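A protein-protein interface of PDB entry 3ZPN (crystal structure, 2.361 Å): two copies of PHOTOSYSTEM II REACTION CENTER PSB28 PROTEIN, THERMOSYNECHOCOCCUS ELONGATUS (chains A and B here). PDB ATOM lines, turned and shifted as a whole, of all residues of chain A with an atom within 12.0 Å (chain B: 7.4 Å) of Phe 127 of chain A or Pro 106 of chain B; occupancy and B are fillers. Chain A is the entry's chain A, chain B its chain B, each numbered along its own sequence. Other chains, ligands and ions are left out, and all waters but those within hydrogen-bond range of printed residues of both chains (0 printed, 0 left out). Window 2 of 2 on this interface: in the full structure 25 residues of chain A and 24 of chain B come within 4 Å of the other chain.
CA of Gly 124 of chain A touches NE1 of Trp 109 of chain B (3.2 Å).
CA of Leu 125 of chain A touches O of Gly 46 of chain B, at 3.3 Å.
Leu 125 of chain A touches Ser 48 of chain B.
Leu 125 of chain A touches Met 103 of chain B (CD1 to O, 3.6 Å).
CD1 of Leu 125 of chain A touches O of Ser 105 of chain B, 3.5 Å away.
Leu 125 of chain A touches Pro 106 of chain B (O to CG, 3.5 Å).
CG of Leu 125 of chain A touches CB of Trp 109 of chain B (3.8 Å).
Gly 126 of chain A touches Pro 106 of chain B.
Phe 127 of chain A touches Pro 106 of chain B (CE2 to CG, 3.9 Å).
N of Ser 105 of chain B lies within hydrogen-bond range of OE1 of Glu 108 of chain B, at 3.2 Å.
No position is printed for both chains.
Printed residues of chain B within 4 Å of Ala 120 of chain A: Trp 109 (2.9 Å).
Ala 121 of chain A touches none of the printed residues of chain B.
Printed residues of chain B within 4 Å of Gly 126 of chain A: Gly 46 (2.8 Å) and Pro 106 (3.7 Å).
Phe 127 of chain A touches just one residue of chain B: Pro 106.
Ser 47 of chain B touches none of the printed residues of chain A.
Of the printed residues of chain A, Ser 105 of chain B touches Leu 125.
Of chain A, only Leu 125 (3.5 Å), Gly 126 (3.7 Å) and Phe 127 (3.9 Å) come within 4 Å of Pro 106 of chain B.
No residue of chain A comes within 4 Å of Gln 107 of chain B.
The nearest residue of chain B that does not touch Phe 127 of chain A is Ser 47 of chain B (4.3 Å).
Hydrophobic or aromatic side chains of chain B within 4 Å of the printed part of chain A: Pro 106 and Trp 109.
Hydrophobic or aromatic side chains of chain A within 4 Å of the printed part of chain B: Leu 125 and Phe 127.
Among the printed residues, no Asp or Glu carboxylate lies within 4 Å of a Lys or Arg side-chain nitrogen of the other chain.
N of Gly 126 of chain A is in hydrogen-bond range of O of Gly 46 of chain B, at 2.8 Å.
O of Ala 120 of chain A is in hydrogen-bond range of NE1 of Trp 109 of chain B (2.9 Å).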
ATOM      1  N   ASP A 117      17.495 -19.222   0.884  1.00  0.00           N
ATOM      2  CA  ASP A 117      16.397 -18.321   0.581  1.00  0.00           C
ATOM      3  C   ASP A 117      15.218 -19.085   0.007  1.00  0.00           C
ATOM      4  O   ASP A 117      14.085 -18.962   0.493  1.00  0.00           O
ATOM      5  CB  ASP A 117      16.842 -17.243  -0.407  1.00  0.00           C
ATOM      6  CG  ASP A 117      15.728 -16.224  -0.726  1.00  0.00           C
ATOM      7  OD1 ASP A 117      15.330 -15.436   0.154  1.00  0.00           O
ATOM      8  OD2 ASP A 117      15.241 -16.210  -1.874  1.00  0.00           O
ATOM      9  N   TYR A 119      14.623 -22.279   0.109  1.00  0.00           N
ATOM     10  CA  TYR A 119      14.100 -23.264   1.033  1.00  0.00           C
ATOM     11  C   TYR A 119      13.214 -22.585   2.067  1.00  0.00           C
ATOM     12  O   TYR A 119      12.063 -22.992   2.278  1.00  0.00           O
ATOM     13  CB  TYR A 119      15.216 -24.070   1.713  1.00  0.00           C
ATOM     14  CG  TYR A 119      14.671 -25.049   2.729  1.00  0.00           C
ATOM     15  CD1 TYR A 119      14.267 -26.322   2.346  1.00  0.00           C
ATOM     16  CD2 TYR A 119      14.530 -24.690   4.063  1.00  0.00           C
ATOM     17  CE1 TYR A 119      13.742 -27.221   3.267  1.00  0.00           C
ATOM     18  CE2 TYR A 119      13.993 -25.578   4.997  1.00  0.00           C
ATOM     19  CZ  TYR A 119      13.607 -26.843   4.596  1.00  0.00           C
ATOM     20  OH  TYR A 119      13.083 -27.724   5.525  1.00  0.00           O
ATOM     21  N   ALA A 120      13.752 -21.548   2.705  1.00  0.00           N
ATOM     22  CA  ALA A 120      13.023 -20.868   3.762  1.00  0.00           C
ATOM     23  C   ALA A 120      11.757 -20.195   3.230  1.00  0.00           C
ATOM     24  O   ALA A 120      10.711 -20.234   3.888  1.00  0.00           O
ATOM     25  CB  ALA A 120      13.921 -19.877   4.481  1.00  0.00           C
ATOM     26  N   ALA A 121      11.821 -19.677   2.003  1.00  0.00           N
ATOM     27  CA  ALA A 121      10.656 -19.046   1.380  1.00  0.00           C
ATOM     28  C   ALA A 121       9.554 -20.050   1.044  1.00  0.00           C
ATOM     29  O   ALA A 121       8.392 -19.692   1.080  1.00  0.00           O
ATOM     30  CB  ALA A 121      11.063 -18.247   0.134  1.00  0.00           C
ATOM     31  N   SER A 122       9.916 -21.296   0.715  1.00  0.00           N
ATOM     32  CA  SER A 122       8.907 -22.321   0.388  1.00  0.00           C
ATOM     33  C   SER A 122       8.513 -23.198   1.580  1.00  0.00           C
ATOM     34  O   SER A 122       7.672 -24.079   1.478  1.00  0.00           O
ATOM     35  CB  SER A 122       9.386 -23.209  -0.765  1.00  0.00           C
ATOM     36  OG  SER A 122      10.566 -23.890  -0.442  1.00  0.00           O
ATOM     37  N   HIS A 123       9.211 -23.010   2.681  1.00  0.00           N
ATOM     38  CA  HIS A 123       8.926 -23.664   3.960  1.00  0.00           C
ATOM     39  C   HIS A 123       8.284 -22.783   5.050  1.00  0.00           C
ATOM     40  O   HIS A 123       8.559 -22.985   6.237  1.00  0.00           O
ATOM     41  CB  HIS A 123      10.076 -24.584   4.397  1.00  0.00           C
ATOM     42  CG  HIS A 123      10.316 -25.699   3.426  1.00  0.00           C
ATOM     43  ND1 HIS A 123      10.847 -25.488   2.166  1.00  0.00           N
ATOM     44  CD2 HIS A 123      10.066 -27.031   3.508  1.00  0.00           C
ATOM     45  CE1 HIS A 123      10.918 -26.639   1.519  1.00  0.00           C
ATOM     46  NE2 HIS A 123      10.461 -27.592   2.312  1.00  0.00           N
ATOM     47  N   GLY A 124       7.663 -21.677   4.644  1.00  0.00           N
ATOM     48  CA  GLY A 124       7.139 -20.697   5.590  1.00  0.00           C
ATOM     49  C   GLY A 124       5.897 -21.036   6.408  1.00  0.00           C
ATOM     50  O   GLY A 124       5.546 -22.204   6.585  1.00  0.00           O
ATOM     51  N   LEU A 125       5.287 -19.995   6.980  1.00  0.00           N
ATOM     52  CA  LEU A 125       4.169 -20.122   7.923  1.00  0.00           C
ATOM     53  C   LEU A 125       2.764 -20.301   7.326  1.00  0.00           C
ATOM     54  O   LEU A 125       2.476 -19.871   6.195  1.00  0.00           O
ATOM     55  CB  LEU A 125       4.152 -18.931   8.884  1.00  0.00           C
ATOM     56  CG  LEU A 125       5.436 -18.642   9.657  1.00  0.00           C
ATOM     57  CD1 LEU A 125       5.239 -17.487  10.624  1.00  0.00           C
ATOM     58  CD2 LEU A 125       5.891 -19.876  10.390  1.00  0.00           C
ATOM     59  N   GLY A 126       1.897 -20.929   8.123  1.00  0.00           N
ATOM     60  CA  GLY A 126       0.478 -21.059   7.822  1.00  0.00           C
ATOM     61  C   GLY A 126      -0.303 -20.210   8.814  1.00  0.00           C
ATOM     62  O   GLY A 126       0.251 -19.257   9.367  1.00  0.00           O
ATOM     63  N   PHE A 127      -1.573 -20.533   9.061  1.00  0.00           N
ATOM     64  CA  PHE A 127      -2.369 -19.713   9.985  1.00  0.00           C
ATOM     65  C   PHE A 127      -2.700 -20.407  11.297  1.00  0.00           C
ATOM     66  O   PHE A 127      -2.407 -19.875  12.365  1.00  0.00           O
ATOM     67  CB  PHE A 127      -3.634 -19.167   9.314  1.00  0.00           C
ATOM     68  CG  PHE A 127      -3.392 -17.919   8.489  1.00  0.00           C
ATOM     69  CD1 PHE A 127      -3.366 -16.659   9.093  1.00  0.00           C
ATOM     70  CD2 PHE A 127      -3.185 -18.002   7.111  1.00  0.00           C
ATOM     71  CE1 PHE A 127      -3.145 -15.500   8.334  1.00  0.00           C
ATOM     72  CE2 PHE A 127      -2.961 -16.850   6.350  1.00  0.00           C
ATOM     73  CZ  PHE A 127      -2.943 -15.599   6.963  1.00  0.00           C
ATOM     74  N   ASP B  45       3.696 -26.680  14.201  1.00  0.00           N
ATOM     75  CA  ASP B  45       2.441 -26.634  13.478  1.00  0.00           C
ATOM     76  C   ASP B  45       2.495 -25.615  12.353  1.00  0.00           C
ATOM     77  O   ASP B  45       1.511 -25.418  11.654  1.00  0.00           O
ATOM     78  CB  ASP B  45       1.283 -26.330  14.430  1.00  0.00           C
ATOM     79  CG  ASP B  45       1.492 -25.028  15.186  1.00  0.00           C
ATOM     80  OD1 ASP B  45       2.585 -24.435  15.033  1.00  0.00           O
ATOM     81  OD2 ASP B  45       0.582 -24.589  15.934  1.00  0.00           O
ATOM     82  N   GLY B  46       3.640 -24.955  12.208  1.00  0.00           N
ATOM     83  CA  GLY B  46       3.844 -23.973  11.157  1.00  0.00           C
ATOM     84  C   GLY B  46       3.166 -22.644  11.446  1.00  0.00           C
ATOM     85  O   GLY B  46       3.070 -21.790  10.570  1.00  0.00           O
ATOM     86  N   SER B  47       2.696 -22.468  12.676  1.00  0.00           N
ATOM     87  CA  SER B  47       1.940 -21.273  13.068  1.00  0.00           C
ATOM     88  C   SER B  47       2.805 -20.031  13.327  1.00  0.00           C
ATOM     89  O   SER B  47       2.370 -18.901  13.083  1.00  0.00           O
ATOM     90  CB  SER B  47       1.057 -21.581  14.286  1.00  0.00           C
ATOM     91  OG  SER B  47       1.815 -22.117  15.371  1.00  0.00           O
ATOM     92  N   SER B  48       4.019 -20.247  13.832  1.00  0.00           N
ATOM     93  CA  SER B  48       4.948 -19.158  14.169  1.00  0.00           C
ATOM     94  C   SER B  48       6.419 -19.517  13.879  1.00  0.00           C
ATOM     95  O   SER B  48       6.748 -20.687  13.675  1.00  0.00           O
ATOM     96  CB  SER B  48       4.787 -18.766  15.642  1.00  0.00           C
ATOM     97  OG  SER B  48       5.178 -19.847  16.461  1.00  0.00           O
ATOM     98  N   MET B 103       7.937 -14.095  14.580  1.00  0.00           N
ATOM     99  CA  MET B 103       7.062 -13.912  13.436  1.00  0.00           C
ATOM    100  C   MET B 103       5.780 -14.693  13.626  1.00  0.00           C
ATOM    101  O   MET B 103       5.809 -15.917  13.833  1.00  0.00           O
ATOM    102  CB  MET B 103       7.787 -14.367  12.177  1.00  0.00           C
ATOM    103  CG  MET B 103       8.916 -13.433  11.800  1.00  0.00           C
ATOM    104  SD  MET B 103      10.258 -14.222  10.879  1.00  0.00           S
ATOM    105  CE  MET B 103      11.055 -15.163  12.202  1.00  0.00           C
ATOM    106  N   ARG B 104       4.660 -13.979  13.624  1.00  0.00           N
ATOM    107  CA  ARG B 104       3.349 -14.603  13.797  1.00  0.00           C
ATOM    108  C   ARG B 104       2.450 -14.767  12.552  1.00  0.00           C
ATOM    109  O   ARG B 104       1.310 -15.198  12.675  1.00  0.00           O
ATOM    110  CB  ARG B 104       2.635 -13.961  14.976  1.00  0.00           C
ATOM    111  CG  ARG B 104       3.513 -14.019  16.237  1.00  0.00           C
ATOM    112  CD  ARG B 104       2.816 -13.519  17.491  1.00  0.00           C
ATOM    113  NE  ARG B 104       3.775 -12.943  18.432  1.00  0.00           N
ATOM    114  CZ  ARG B 104       4.380 -13.616  19.410  1.00  0.00           C
ATOM    115  NH1 ARG B 104       4.146 -14.917  19.583  1.00  0.00           N
ATOM    116  NH2 ARG B 104       5.238 -12.987  20.206  1.00  0.00           N
ATOM    117  N   SER B 105       2.930 -14.377  11.374  1.00  0.00           N
ATOM    118  CA  SER B 105       2.128 -14.506  10.149  1.00  0.00           C
ATOM    119  C   SER B 105       3.006 -14.822   8.941  1.00  0.00           C
ATOM    120  O   SER B 105       4.214 -14.588   8.969  1.00  0.00           O
ATOM    121  CB  SER B 105       1.316 -13.233   9.890  1.00  0.00           C
ATOM    122  OG  SER B 105       2.131 -12.170   9.441  1.00  0.00           O
ATOM    123  N   PRO B 106       2.403 -15.395   7.884  1.00  0.00           N
ATOM    124  CA  PRO B 106       3.110 -15.623   6.613  1.00  0.00           C
ATOM    125  C   PRO B 106       3.821 -14.380   6.073  1.00  0.00           C
ATOM    126  O   PRO B 106       4.962 -14.465   5.615  1.00  0.00           O
ATOM    127  CB  PRO B 106       1.974 -16.038   5.668  1.00  0.00           C
ATOM    128  CG  PRO B 106       0.977 -16.715   6.558  1.00  0.00           C
ATOM    129  CD  PRO B 106       1.052 -16.000   7.887  1.00  0.00           C
ATOM    130  N   GLN B 107       3.164 -13.233   6.167  1.00  0.00           N
ATOM    131  CA  GLN B 107       3.722 -11.969   5.707  1.00  0.00           C
ATOM    132  C   GLN B 107       4.992 -11.594   6.480  1.00  0.00           C
ATOM    133  O   GLN B 107       5.957 -11.108   5.900  1.00  0.00           O
ATOM    134  CB  GLN B 107       2.666 -10.870   5.836  1.00  0.00           C
ATOM    135  CG  GLN B 107       3.125  -9.493   5.441  1.00  0.00           C
ATOM    136  CD  GLN B 107       2.034  -8.442   5.635  1.00  0.00           C
ATOM    137  OE1 GLN B 107       0.881  -8.780   5.920  1.00  0.00           O
ATOM    138  NE2 GLN B 107       2.395  -7.163   5.480  1.00  0.00           N
ATOM    139  N   GLU B 108       4.984 -11.794   7.793  1.00  0.00           N
ATOM    140  CA  GLU B 108       6.150 -11.457   8.611  1.00  0.00           C
ATOM    141  C   GLU B 108       7.340 -12.381   8.295  1.00  0.00           C
ATOM    142  O   GLU B 108       8.481 -11.917   8.129  1.00  0.00           O
ATOM    143  CB  GLU B 108       5.802 -11.512  10.098  1.00  0.00           C
ATOM    144  CG  GLU B 108       4.842 -10.416  10.578  1.00  0.00           C
ATOM    145  CD  GLU B 108       4.424 -10.606  12.036  1.00  0.00           C
ATOM    146  OE1 GLU B 108       4.373 -11.759  12.518  1.00  0.00           O
ATOM    147  OE2 GLU B 108       4.155  -9.600  12.713  1.00  0.00           O
ATOM    148  N   TRP B 109       7.054 -13.670   8.154  1.00  0.00           N
ATOM    149  CA  TRP B 109       8.061 -14.640   7.759  1.00  0.00           C
ATOM    150  C   TRP B 109       8.655 -14.287   6.394  1.00  0.00           C
ATOM    151  O   TRP B 109       9.880 -14.279   6.245  1.00  0.00           O
ATOM    152  CB  TRP B 109       7.468 -16.045   7.738  1.00  0.00           C
ATOM    153  CG  TRP B 109       8.422 -17.130   7.313  1.00  0.00           C
ATOM    154  CD1 TRP B 109       8.661 -17.554   6.041  1.00  0.00           C
ATOM    155  CD2 TRP B 109       9.224 -17.965   8.169  1.00  0.00           C
ATOM    156  NE1 TRP B 109       9.564 -18.586   6.044  1.00  0.00           N
ATOM    157  CE2 TRP B 109       9.939 -18.853   7.335  1.00  0.00           C
ATOM    158  CE3 TRP B 109       9.411 -18.043   9.555  1.00  0.00           C
ATOM    159  CZ2 TRP B 109      10.822 -19.813   7.834  1.00  0.00           C
ATOM    160  CZ3 TRP B 109      10.298 -19.000  10.056  1.00  0.00           C
ATOM    161  CH2 TRP B 109      10.991 -19.872   9.192  1.00  0.00           C
ATOM    162  N   ASP B 110       7.800 -13.999   5.406  1.00  0.00           N
ATOM    163  CA  ASP B 110       8.285 -13.657   4.070  1.00  0.00           C
ATOM    164  C   ASP B 110       9.094 -12.343   4.048  1.00  0.00           C
ATOM    165  O   ASP B 110      10.120 -12.241   3.362  1.00  0.00           O
ATOM    166  CB  ASP B 110       7.135 -13.563   3.059  1.00  0.00           C
ATOM    167  CG  ASP B 110       6.468 -14.900   2.800  1.00  0.00           C
ATOM    168  OD1 ASP B 110       7.082 -15.962   3.063  1.00  0.00           O
ATOM    169  OD2 ASP B 110       5.326 -14.889   2.299  1.00  0.00           O
ATOM    170  N   ARG B 111       8.642 -11.355   4.814  1.00  0.00           N
ATOM    171  CA  ARG B 111       9.328 -10.073   4.895  1.00  0.00           C
ATOM    172  C   ARG B 111      10.698 -10.287   5.497  1.00  0.00           C
ATOM    173  O   ARG B 111      11.684  -9.696   5.053  1.00  0.00           O
ATOM    174  CB  ARG B 111       8.531  -9.101   5.768  1.00  0.00           C
ATOM    175  CG  ARG B 111       9.274  -7.850   6.214  1.00  0.00           C
ATOM    176  CD  ARG B 111       9.569  -6.945   5.031  1.00  0.00           C
ATOM    177  NE  ARG B 111      10.278  -5.732   5.435  1.00  0.00           N
ATOM    178  CZ  ARG B 111      11.564  -5.513   5.216  1.00  0.00           C
ATOM    179  NH1 ARG B 111      12.286  -6.424   4.588  1.00  0.00           N
ATOM    180  NH2 ARG B 111      12.121  -4.376   5.611  1.00  0.00           N
ATOM    181  N   PHE B 112      10.765 -11.163   6.495  1.00  0.00           N
ATOM    182  CA  PHE B 112      12.024 -11.357   7.190  1.00  0.00           C
ATOM    183  C   PHE B 112      13.048 -12.108   6.383  1.00  0.00           C
ATOM    184  O   PHE B 112      14.244 -11.822   6.464  1.00  0.00           O
ATOM    185  CB  PHE B 112      11.847 -12.062   8.518  1.00  0.00           C
ATOM    186  CG  PHE B 112      13.147 -12.446   9.139  1.00  0.00           C
ATOM    187  CD1 PHE B 112      13.961 -11.478   9.716  1.00  0.00           C
ATOM    188  CD2 PHE B 112      13.568 -13.756   9.143  1.00  0.00           C
ATOM    189  CE1 PHE B 112      15.179 -11.810  10.294  1.00  0.00           C
ATOM    190  CE2 PHE B 112      14.788 -14.108   9.726  1.00  0.00           C
ATOM    191  CZ  PHE B 112      15.597 -13.122  10.304  1.00  0.00           C
ATOM    192  N   ARG B 114      13.295 -12.075   3.152  1.00  0.00           N
ATOM    193  CA  ARG B 114      13.804 -11.136   2.159  1.00  0.00           C
ATOM    194  C   ARG B 114      14.935 -10.297   2.741  1.00  0.00           C
ATOM    195  O   ARG B 114      15.985 -10.163   2.117  1.00  0.00           O
ATOM    196  CB  ARG B 114      12.685 -10.228   1.602  1.00  0.00           C
ATOM    197  CG  ARG B 114      11.608 -10.962   0.784  1.00  0.00           C
ATOM    198  CD  ARG B 114      10.751 -10.017  -0.085  1.00  0.00           C
ATOM    199  NE  ARG B 114      10.022  -8.995   0.686  1.00  0.00           N
ATOM    200  CZ  ARG B 114       8.858  -9.183   1.320  1.00  0.00           C
ATOM    201  NH1 ARG B 114       8.254 -10.379   1.342  1.00  0.00           N
ATOM    202  NH2 ARG B 114       8.308  -8.162   1.966  1.00  0.00           N
